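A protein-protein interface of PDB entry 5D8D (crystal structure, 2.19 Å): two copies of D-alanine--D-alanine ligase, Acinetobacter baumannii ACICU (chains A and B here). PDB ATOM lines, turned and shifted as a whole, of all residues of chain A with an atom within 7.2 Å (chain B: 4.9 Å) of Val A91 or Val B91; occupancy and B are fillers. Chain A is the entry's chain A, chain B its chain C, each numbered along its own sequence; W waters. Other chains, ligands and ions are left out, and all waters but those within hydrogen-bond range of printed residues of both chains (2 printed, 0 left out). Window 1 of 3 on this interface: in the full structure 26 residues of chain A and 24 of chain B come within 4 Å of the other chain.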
ATOM      1  N   GLU A  71      23.800   1.618 -18.237  1.00  0.00           N
ATOM      2  CA  GLU A  71      23.200   2.925 -18.307  1.00  0.00           C
ATOM      3  C   GLU A  71      22.374   3.129 -19.612  1.00  0.00           C
ATOM      4  O   GLU A  71      21.700   4.133 -19.775  1.00  0.00           O
ATOM      5  CB  GLU A  71      24.394   3.883 -18.277  1.00  0.00           C
ATOM      6  CG  GLU A  71      24.144   5.320 -17.889  1.00  0.00           C
ATOM      7  CD  GLU A  71      25.444   6.106 -17.781  1.00  0.00           C
ATOM      8  OE1 GLU A  71      25.431   7.287 -18.205  1.00  0.00           O
ATOM      9  OE2 GLU A  71      26.473   5.547 -17.298  1.00  0.00           O
ATOM     10  N   ASP A  72      22.422   2.164 -20.518  1.00  0.00           N
ATOM     11  CA  ASP A  72      21.865   2.268 -21.886  1.00  0.00           C
ATOM     12  C   ASP A  72      20.606   1.416 -22.170  1.00  0.00           C
ATOM     13  O   ASP A  72      20.240   1.246 -23.337  1.00  0.00           O
ATOM     14  CB  ASP A  72      22.950   1.862 -22.889  1.00  0.00           C
ATOM     15  CG  ASP A  72      23.455   0.448 -22.649  1.00  0.00           C
ATOM     16  OD1 ASP A  72      22.897  -0.266 -21.777  1.00  0.00           O
ATOM     17  OD2 ASP A  72      24.422   0.054 -23.322  1.00  0.00           O
ATOM     18  N   GLY A  73      19.981   0.878 -21.121  1.00  0.00           N
ATOM     19  CA  GLY A  73      18.720   0.110 -21.247  1.00  0.00           C
ATOM     20  C   GLY A  73      18.892  -1.413 -21.289  1.00  0.00           C
ATOM     21  O   GLY A  73      17.931  -2.146 -21.141  1.00  0.00           O
ATOM     22  N   GLN A  74      20.124  -1.890 -21.418  1.00  0.00           N
ATOM     23  CA  GLN A  74      20.359  -3.290 -21.504  1.00  0.00           C
ATOM     24  C   GLN A  74      20.094  -4.052 -20.204  1.00  0.00           C
ATOM     25  O   GLN A  74      19.362  -5.027 -20.190  1.00  0.00           O
ATOM     26  CB  GLN A  74      21.797  -3.533 -21.891  1.00  0.00           C
ATOM     27  CG  GLN A  74      22.153  -3.012 -23.265  1.00  0.00           C
ATOM     28  CD  GLN A  74      23.444  -3.558 -23.785  1.00  0.00           C
ATOM     29  OE1 GLN A  74      23.901  -3.111 -24.809  1.00  0.00           O
ATOM     30  NE2 GLN A  74      23.997  -4.572 -23.143  1.00  0.00           N
ATOM     31  N   ILE A  75      20.715  -3.639 -19.114  1.00  0.00           N
ATOM     32  CA  ILE A  75      20.512  -4.350 -17.866  1.00  0.00           C
ATOM     33  C   ILE A  75      19.076  -4.115 -17.396  1.00  0.00           C
ATOM     34  O   ILE A  75      18.502  -4.998 -16.772  1.00  0.00           O
ATOM     35  CB  ILE A  75      21.559  -3.986 -16.776  1.00  0.00           C
ATOM     36  CG1 ILE A  75      21.525  -4.959 -15.571  1.00  0.00           C
ATOM     37  CG2 ILE A  75      21.323  -2.569 -16.246  1.00  0.00           C
ATOM     38  CD1 ILE A  75      21.939  -6.383 -15.853  1.00  0.00           C
ATOM     39  N   GLN A  76      18.503  -2.941 -17.688  1.00  0.00           N
ATOM     40  CA  GLN A  76      17.093  -2.644 -17.332  1.00  0.00           C
ATOM     41  C   GLN A  76      16.146  -3.544 -18.159  1.00  0.00           C
ATOM     42  O   GLN A  76      15.113  -3.992 -17.681  1.00  0.00           O
ATOM     43  CB  GLN A  76      16.760  -1.196 -17.630  1.00  0.00           C
ATOM     44  CG  GLN A  76      17.463  -0.117 -16.792  1.00  0.00           C
ATOM     45  CD  GLN A  76      18.941   0.033 -17.074  1.00  0.00           C
ATOM     46  OE1 GLN A  76      19.445  -0.479 -18.043  1.00  0.00           O
ATOM     47  NE2 GLN A  76      19.639   0.715 -16.213  1.00  0.00           N
ATOM     48  N   GLY A  77      16.532  -3.816 -19.409  1.00  0.00           N
ATOM     49  CA  GLY A  77      15.851  -4.795 -20.256  1.00  0.00           C
ATOM     50  C   GLY A  77      15.724  -6.144 -19.578  1.00  0.00           C
ATOM     51  O   GLY A  77      14.596  -6.699 -19.458  1.00  0.00           O
ATOM     52  N   VAL A  78      16.858  -6.667 -19.092  1.00  0.00           N
ATOM     53  CA  VAL A  78      16.816  -7.996 -18.433  1.00  0.00           C
ATOM     54  C   VAL A  78      15.978  -7.966 -17.168  1.00  0.00           C
ATOM     55  O   VAL A  78      15.231  -8.908 -16.879  1.00  0.00           O
ATOM     56  CB  VAL A  78      18.182  -8.773 -18.238  1.00  0.00           C
ATOM     57  CG1 VAL A  78      19.317  -8.289 -19.144  1.00  0.00           C
ATOM     58  CG2 VAL A  78      18.604  -8.877 -16.800  1.00  0.00           C
ATOM     59  N   LEU A  79      16.073  -6.878 -16.439  1.00  0.00           N
ATOM     60  CA  LEU A  79      15.356  -6.783 -15.202  1.00  0.00           C
ATOM     61  C   LEU A  79      13.855  -6.726 -15.448  1.00  0.00           C
ATOM     62  O   LEU A  79      13.106  -7.358 -14.714  1.00  0.00           O
ATOM     63  CB  LEU A  79      15.835  -5.585 -14.387  1.00  0.00           C
ATOM     64  CG  LEU A  79      17.236  -5.756 -13.829  1.00  0.00           C
ATOM     65  CD1 LEU A  79      17.706  -4.404 -13.415  1.00  0.00           C
ATOM     66  CD2 LEU A  79      17.278  -6.700 -12.626  1.00  0.00           C
ATOM     67  N   GLU A  80      13.422  -5.974 -16.460  1.00  0.00           N
ATOM     68  CA  GLU A  80      12.007  -5.969 -16.874  1.00  0.00           C
ATOM     69  C   GLU A  80      11.546  -7.391 -17.267  1.00  0.00           C
ATOM     70  O   GLU A  80      10.527  -7.863 -16.763  1.00  0.00           O
ATOM     71  CB  GLU A  80      11.778  -5.010 -18.047  1.00  0.00           C
ATOM     72  CG  GLU A  80      11.940  -3.518 -17.747  1.00  0.00           C
ATOM     73  CD  GLU A  80      10.891  -2.977 -16.803  1.00  0.00           C
ATOM     74  OE1 GLU A  80       9.883  -3.675 -16.571  1.00  0.00           O
ATOM     75  OE2 GLU A  80      11.090  -1.854 -16.275  1.00  0.00           O
ATOM     76  N   TYR A  86      13.772  -2.401  -9.774  1.00  0.00           N
ATOM     77  CA  TYR A  86      15.139  -1.915  -9.748  1.00  0.00           C
ATOM     78  C   TYR A  86      15.192  -0.386  -9.657  1.00  0.00           C
ATOM     79  O   TYR A  86      14.189   0.279  -9.784  1.00  0.00           O
ATOM     80  CB  TYR A  86      15.916  -2.456 -10.964  1.00  0.00           C
ATOM     81  CG  TYR A  86      15.339  -2.013 -12.259  1.00  0.00           C
ATOM     82  CD1 TYR A  86      15.684  -0.766 -12.819  1.00  0.00           C
ATOM     83  CD2 TYR A  86      14.422  -2.803 -12.929  1.00  0.00           C
ATOM     84  CE1 TYR A  86      15.139  -0.329 -14.005  1.00  0.00           C
ATOM     85  CE2 TYR A  86      13.838  -2.366 -14.124  1.00  0.00           C
ATOM     86  CZ  TYR A  86      14.210  -1.131 -14.648  1.00  0.00           C
ATOM     87  OH  TYR A  86      13.657  -0.727 -15.806  1.00  0.00           O
ATOM     88  N   THR A  89      16.234   4.929 -13.772  1.00  0.00           N
ATOM     89  CA  THR A  89      15.455   5.058 -14.978  1.00  0.00           C
ATOM     90  C   THR A  89      15.163   3.706 -15.685  1.00  0.00           C
ATOM     91  O   THR A  89      15.942   2.763 -15.579  1.00  0.00           O
ATOM     92  CB  THR A  89      16.143   6.035 -15.936  1.00  0.00           C
ATOM     93  OG1 THR A  89      16.332   7.286 -15.272  1.00  0.00           O
ATOM     94  CG2 THR A  89      15.310   6.266 -17.162  1.00  0.00           C
ATOM     95  N   GLY A  90      14.038   3.630 -16.407  1.00  0.00           N
ATOM     96  CA  GLY A  90      13.646   2.401 -17.163  1.00  0.00           C
ATOM     97  C   GLY A  90      14.439   2.262 -18.451  1.00  0.00           C
ATOM     98  O   GLY A  90      15.373   3.023 -18.725  1.00  0.00           O
ATOM     99  N   VAL A  91      14.020   1.311 -19.269  1.00  0.00           N
ATOM    100  CA  VAL A  91      14.665   1.015 -20.565  1.00  0.00           C
ATOM    101  C   VAL A  91      14.683   2.227 -21.472  1.00  0.00           C
ATOM    102  O   VAL A  91      15.738   2.609 -22.013  1.00  0.00           O
ATOM    103  CB  VAL A  91      13.957  -0.156 -21.302  1.00  0.00           C
ATOM    104  CG1 VAL A  91      14.691  -0.519 -22.597  1.00  0.00           C
ATOM    105  CG2 VAL A  91      13.935  -1.397 -20.412  1.00  0.00           C
ATOM    106  N   GLN A  92      13.517   2.816 -21.689  1.00  0.00           N
ATOM    107  CA  GLN A  92      13.446   3.924 -22.670  1.00  0.00           C
ATOM    108  C   GLN A  92      14.331   5.154 -22.319  1.00  0.00           C
ATOM    109  O   GLN A  92      15.214   5.604 -23.113  1.00  0.00           O
ATOM    110  CB  GLN A  92      12.001   4.360 -22.867  1.00  0.00           C
ATOM    111  CG  GLN A  92      11.883   5.459 -23.891  1.00  0.00           C
ATOM    112  CD  GLN A  92      10.461   5.819 -24.134  1.00  0.00           C
ATOM    113  OE1 GLN A  92       9.776   6.305 -23.257  1.00  0.00           O
ATOM    114  NE2 GLN A  92      10.005   5.563 -25.322  1.00  0.00           N
ATOM    115  N   GLY A  93      14.112   5.658 -21.112  1.00  0.00           N
ATOM    116  CA  GLY A  93      14.878   6.772 -20.593  1.00  0.00           C
ATOM    117  C   GLY A  93      16.393   6.541 -20.566  1.00  0.00           C
ATOM    118  O   GLY A  93      17.183   7.462 -20.832  1.00  0.00           O
ATOM    119  N   SER A  94      16.790   5.325 -20.228  1.00  0.00           N
ATOM    120  CA  SER A  94      18.191   4.982 -20.159  1.00  0.00           C
ATOM    121  C   SER A  94      18.791   4.999 -21.525  1.00  0.00           C
ATOM    122  O   SER A  94      19.815   5.645 -21.722  1.00  0.00           O
ATOM    123  CB  SER A  94      18.420   3.591 -19.513  1.00  0.00           C
ATOM    124  OG  SER A  94      17.852   3.567 -18.231  1.00  0.00           O
ATOM    125  N   ALA A  95      18.159   4.307 -22.469  1.00  0.00           N
ATOM    126  CA  ALA A  95      18.646   4.318 -23.861  1.00  0.00           C
ATOM    127  C   ALA A  95      18.644   5.706 -24.514  1.00  0.00           C
ATOM    128  O   ALA A  95      19.591   6.037 -25.269  1.00  0.00           O
ATOM    129  CB  ALA A  95      17.878   3.353 -24.712  1.00  0.00           C
ATOM    130  N   ILE A  96      17.637   6.527 -24.217  1.00  0.00           N
ATOM    131  CA  ILE A  96      17.716   7.947 -24.639  1.00  0.00           C
ATOM    132  C   ILE A  96      18.874   8.709 -23.927  1.00  0.00           C
ATOM    133  O   ILE A  96      19.714   9.364 -24.588  1.00  0.00           O
ATOM    134  CB  ILE A  96      16.398   8.721 -24.423  1.00  0.00           C
ATOM    135  CG1 ILE A  96      15.264   8.139 -25.282  1.00  0.00           C
ATOM    136  CG2 ILE A  96      16.624  10.184 -24.786  1.00  0.00           C
ATOM    137  CD1 ILE A  96      13.860   8.583 -24.876  1.00  0.00           C
ATOM    138  N   GLY A  97      18.928   8.614 -22.595  1.00  0.00           N
ATOM    139  CA  GLY A  97      19.929   9.323 -21.781  1.00  0.00           C
ATOM    140  C   GLY A  97      21.382   8.986 -22.089  1.00  0.00           C
ATOM    141  O   GLY A  97      22.272   9.777 -21.781  1.00  0.00           O
ATOM    142  N   GLU A 249      13.737   8.534 -13.994  1.00  0.00           N
ATOM    143  CA  GLU A 249      12.965   8.303 -12.748  1.00  0.00           C
ATOM    144  C   GLU A 249      13.899   8.063 -11.595  1.00  0.00           C
ATOM    145  O   GLU A 249      14.979   7.506 -11.787  1.00  0.00           O
ATOM    146  CB  GLU A 249      12.068   7.064 -12.829  1.00  0.00           C
ATOM    147  CG  GLU A 249      10.765   7.199 -13.609  1.00  0.00           C
ATOM    148  CD  GLU A 249      10.033   5.852 -13.637  1.00  0.00           C
ATOM    149  OE1 GLU A 249       9.357   5.509 -12.628  1.00  0.00           O
ATOM    150  OE2 GLU A 249      10.180   5.106 -14.644  1.00  0.00           O
ATOM    151  N   ASP B  72      10.067  -3.596 -27.363  1.00  0.00           N
ATOM    152  CA  ASP B  72      10.411  -2.445 -26.500  1.00  0.00           C
ATOM    153  C   ASP B  72      11.826  -2.562 -25.913  1.00  0.00           C
ATOM    154  O   ASP B  72      12.190  -1.814 -25.043  1.00  0.00           O
ATOM    155  CB  ASP B  72       9.370  -2.252 -25.399  1.00  0.00           C
ATOM    156  CG  ASP B  72       9.176  -3.500 -24.521  1.00  0.00           C
ATOM    157  OD1 ASP B  72       9.839  -4.517 -24.765  1.00  0.00           O
ATOM    158  OD2 ASP B  72       8.325  -3.471 -23.587  1.00  0.00           O
ATOM    159  N   GLY B  73      12.639  -3.489 -26.401  1.00  0.00           N
ATOM    160  CA  GLY B  73      14.008  -3.623 -25.895  1.00  0.00           C
ATOM    161  C   GLY B  73      14.252  -4.611 -24.774  1.00  0.00           C
ATOM    162  O   GLY B  73      15.391  -4.911 -24.527  1.00  0.00           O
ATOM    163  N   GLN B  76      15.775  -7.715 -26.174  1.00  0.00           N
ATOM    164  CA  GLN B  76      17.023  -7.284 -26.805  1.00  0.00           C
ATOM    165  C   GLN B  76      18.113  -7.067 -25.759  1.00  0.00           C
ATOM    166  O   GLN B  76      19.292  -7.445 -25.954  1.00  0.00           O
ATOM    167  CB  GLN B  76      16.830  -6.019 -27.648  1.00  0.00           C
ATOM    168  CG  GLN B  76      16.019  -6.216 -28.919  1.00  0.00           C
ATOM    169  CD  GLN B  76      14.490  -6.332 -28.686  1.00  0.00           C
ATOM    170  OE1 GLN B  76      13.944  -5.992 -27.632  1.00  0.00           O
ATOM    171  NE2 GLN B  76      13.806  -6.823 -29.694  1.00  0.00           N
ATOM    172  N   GLY B  77      17.691  -6.482 -24.644  1.00  0.00           N
ATOM    173  CA  GLY B  77      18.543  -6.348 -23.492  1.00  0.00           C
ATOM    174  C   GLY B  77      19.088  -7.689 -22.995  1.00  0.00           C
ATOM    175  O   GLY B  77      20.293  -7.821 -22.809  1.00  0.00           O
ATOM    176  N   GLU B  80      21.629  -9.028 -25.508  1.00  0.00           N
ATOM    177  CA  GLU B  80      22.877  -8.289 -25.484  1.00  0.00           C
ATOM    178  C   GLU B  80      23.759  -8.886 -24.353  1.00  0.00           C
ATOM    179  O   GLU B  80      24.872  -9.322 -24.597  1.00  0.00           O
ATOM    180  CB  GLU B  80      22.641  -6.807 -25.233  1.00  0.00           C
ATOM    181  CG  GLU B  80      22.004  -6.018 -26.370  1.00  0.00           C
ATOM    182  CD  GLU B  80      22.931  -5.772 -27.560  1.00  0.00           C
ATOM    183  OE1 GLU B  80      24.137  -6.081 -27.492  1.00  0.00           O
ATOM    184  OE2 GLU B  80      22.416  -5.280 -28.595  1.00  0.00           O
ATOM    185  N   TYR B  86      21.302 -11.199 -32.834  1.00  0.00           N
ATOM    186  CA  TYR B  86      19.903 -11.214 -33.070  1.00  0.00           C
ATOM    187  C   TYR B  86      19.454 -10.245 -34.169  1.00  0.00           C
ATOM    188  O   TYR B  86      20.111  -9.276 -34.471  1.00  0.00           O
ATOM    189  CB  TYR B  86      19.165 -10.926 -31.740  1.00  0.00           C
ATOM    190  CG  TYR B  86      19.344  -9.535 -31.150  1.00  0.00           C
ATOM    191  CD1 TYR B  86      18.504  -8.481 -31.522  1.00  0.00           C
ATOM    192  CD2 TYR B  86      20.348  -9.281 -30.201  1.00  0.00           C
ATOM    193  CE1 TYR B  86      18.666  -7.218 -30.986  1.00  0.00           C
ATOM    194  CE2 TYR B  86      20.516  -8.020 -29.644  1.00  0.00           C
ATOM    195  CZ  TYR B  86      19.684  -6.982 -30.041  1.00  0.00           C
ATOM    196  OH  TYR B  86      19.857  -5.741 -29.481  1.00  0.00           O
ATOM    197  N   THR B  89      16.272  -4.295 -34.706  1.00  0.00           N
ATOM    198  CA  THR B  89      16.681  -3.137 -33.941  1.00  0.00           C
ATOM    199  C   THR B  89      17.127  -3.475 -32.502  1.00  0.00           C
ATOM    200  O   THR B  89      16.499  -4.297 -31.810  1.00  0.00           O
ATOM    201  CB  THR B  89      15.518  -2.118 -33.951  1.00  0.00           C
ATOM    202  OG1 THR B  89      15.357  -1.657 -35.296  1.00  0.00           O
ATOM    203  CG2 THR B  89      15.804  -0.941 -33.043  1.00  0.00           C
ATOM    204  N   GLY B  90      18.171  -2.768 -32.055  1.00  0.00           N
ATOM    205  CA  GLY B  90      18.759  -2.935 -30.738  1.00  0.00           C
ATOM    206  C   GLY B  90      17.923  -2.286 -29.660  1.00  0.00           C
ATOM    207  O   GLY B  90      16.827  -1.787 -29.921  1.00  0.00           O
ATOM    208  N   VAL B  91      18.458  -2.266 -28.441  1.00  0.00           N
ATOM    209  CA  VAL B  91      17.692  -1.849 -27.259  1.00  0.00           C
ATOM    210  C   VAL B  91      17.047  -0.485 -27.398  1.00  0.00           C
ATOM    211  O   VAL B  91      15.826  -0.375 -27.173  1.00  0.00           O
ATOM    212  CB  VAL B  91      18.541  -1.890 -26.000  1.00  0.00           C
ATOM    213  CG1 VAL B  91      17.773  -1.336 -24.801  1.00  0.00           C
ATOM    214  CG2 VAL B  91      18.910  -3.327 -25.713  1.00  0.00           C
ATOM    215  N   GLN B  92      17.870   0.499 -27.781  1.00  0.00           N
ATOM    216  CA  GLN B  92      17.488   1.899 -27.902  1.00  0.00           C
ATOM    217  C   GLN B  92      16.380   2.166 -28.931  1.00  0.00           C
ATOM    218  O   GLN B  92      15.402   2.899 -28.659  1.00  0.00           O
ATOM    219  CB  GLN B  92      18.730   2.782 -28.247  1.00  0.00           C
ATOM    220  CG  GLN B  92      18.376   4.284 -28.527  1.00  0.00           C
ATOM    221  CD  GLN B  92      19.515   5.110 -29.129  1.00  0.00           C
ATOM    222  OE1 GLN B  92      19.840   4.994 -30.310  1.00  0.00           O
ATOM    223  NE2 GLN B  92      20.118   5.956 -28.319  1.00  0.00           N
ATOM    224  N   GLY B  93      16.577   1.630 -30.137  1.00  0.00           N
ATOM    225  CA  GLY B  93      15.676   1.862 -31.235  1.00  0.00           C
ATOM    226  C   GLY B  93      14.337   1.287 -30.877  1.00  0.00           C
ATOM    227  O   GLY B  93      13.314   1.917 -31.153  1.00  0.00           O
ATOM    228  N   SER B  94      14.346   0.109 -30.251  1.00  0.00           N
ATOM    229  CA  SER B  94      13.112  -0.586 -29.924  1.00  0.00           C
ATOM    230  C   SER B  94      12.412   0.150 -28.808  1.00  0.00           C
ATOM    231  O   SER B  94      11.206   0.316 -28.828  1.00  0.00           O
ATOM    232  CB  SER B  94      13.323  -2.064 -29.495  1.00  0.00           C
ATOM    233  OG  SER B  94      14.301  -2.701 -30.302  1.00  0.00           O
ATOM    234  N   ALA B  95      13.154   0.583 -27.804  1.00  0.00           N
ATOM    235  CA  ALA B  95      12.515   1.300 -26.693  1.00  0.00           C
ATOM    236  C   ALA B  95      11.835   2.575 -27.180  1.00  0.00           C
ATOM    237  O   ALA B  95      10.779   2.896 -26.716  1.00  0.00           O
ATOM    238  CB  ALA B  95      13.530   1.621 -25.594  1.00  0.00           C
HETATM  239  O   HOH W   1      22.598   5.046 -26.108  1.00  0.00           O
HETATM  240  O   HOH W   2      20.923   0.937 -26.186  1.00  0.00           O
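The backbone carbonyl oxygen (O) of Ala B95 lies within hydrogen-bond range of the side-chain amide nitrogen (NE2) of Gln A92, at 3.1 Å. NE2 of Gln B92 lies within hydrogen-bond range of O of Ala A95 (3.1 Å).
The side-chain carboxylate of Glu B80 lies within hydrogen-bond range of the side-chain hydroxyl of Tyr B86. The side-chain carboxylate (OD1) of Asp A72 lies close to the backbone NH (N) of Gln A74 (3.2 Å). The side-chain amide oxygen (OE1) of Gln A76 lies close to the backbone NH (N) of Gly A73 (3.4 Å).
O of Asp A72 touches CG1 of Val B91, at 3.9 Å. Gly A73 touches Val B91 (C to CG1, 3.7 Å). CA of Gly B77 touches O of Gln A74, at 3.6 Å. Glu B80 touches Gln A74 (CB to NE2, 3.3 Å). CG1 of Val A78 touches O of Gly B77 (3.8 Å). O of Asp B72 touches CG1 of Val A91 (3.7 Å). Val A91 touches Val B91. CG1 of Val A91 touches CB of Ala B95, 3.9 Å away.
Val A91 touches just these residues of chain B: Asp B72, Val B91 and Ala B95. Val B91 touches just these residues of chain A: Asp A72 (3.9 Å), Gly A73 (3.7 Å) and Val A91 (3.9 Å). Of the printed residues of chain B, Gln A74 touches Gly B77 and Glu B80. Printed residues of chain A within 4 Å of Ala B95: Val A91 (3.9 Å) and Gln A92 (3.1 Å). Of the printed residues of chain B, Gly A73 touches Val B91 (3.7 Å).
Of the 13 printed residues of chain B, 6 touch a printed residue of chain A. Hydrophobic or aromatic side chains of chain B that line the printed part of chain A: Val B91 and Ala B95. Of the 21 printed residues of chain A, 7 touch a printed residue of chain B. Printed residues of chain A that touch a printed residue of chain B: Asp A72, Gly A73, Gln A74, Val A78, Val A91, Gln A92 and Ala A95. Hydrophobic or aromatic side chains of chain A within 4 Å of the printed part of chain B: Val A78, Val A91 and Ala A95. Among the printed residues, no Asp or Glu carboxylate lies within 4 Å of a Lys or Arg side-chain nitrogen of the other chain.
Asp A72 touches Val B91, and with the chains exchanged Val A91 touches Asp B72. Gly A73 touches Val B91, but with the chains exchanged Val A91 does not touch Gly B73 (4.6 Å). Val A91 touches its own counterpart, Val B91. Val A91 touches Ala B95, but with the chains exchanged Ala A95 does not touch Val B91 (4.7 Å). Positions printed for both chains: 72, 73, 76, 77, 80, 86, 89, 90, 91, 92, 93, 94 and 95.
Water W2 bridges O of Asp A72 (2.9 Å) and N of Gln B92 (3.5 Å). Water W1 lies within hydrogen-bond range of O of Ala A95 (3.3 Å) and NE2 of Gln B92 (3.4 Å).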
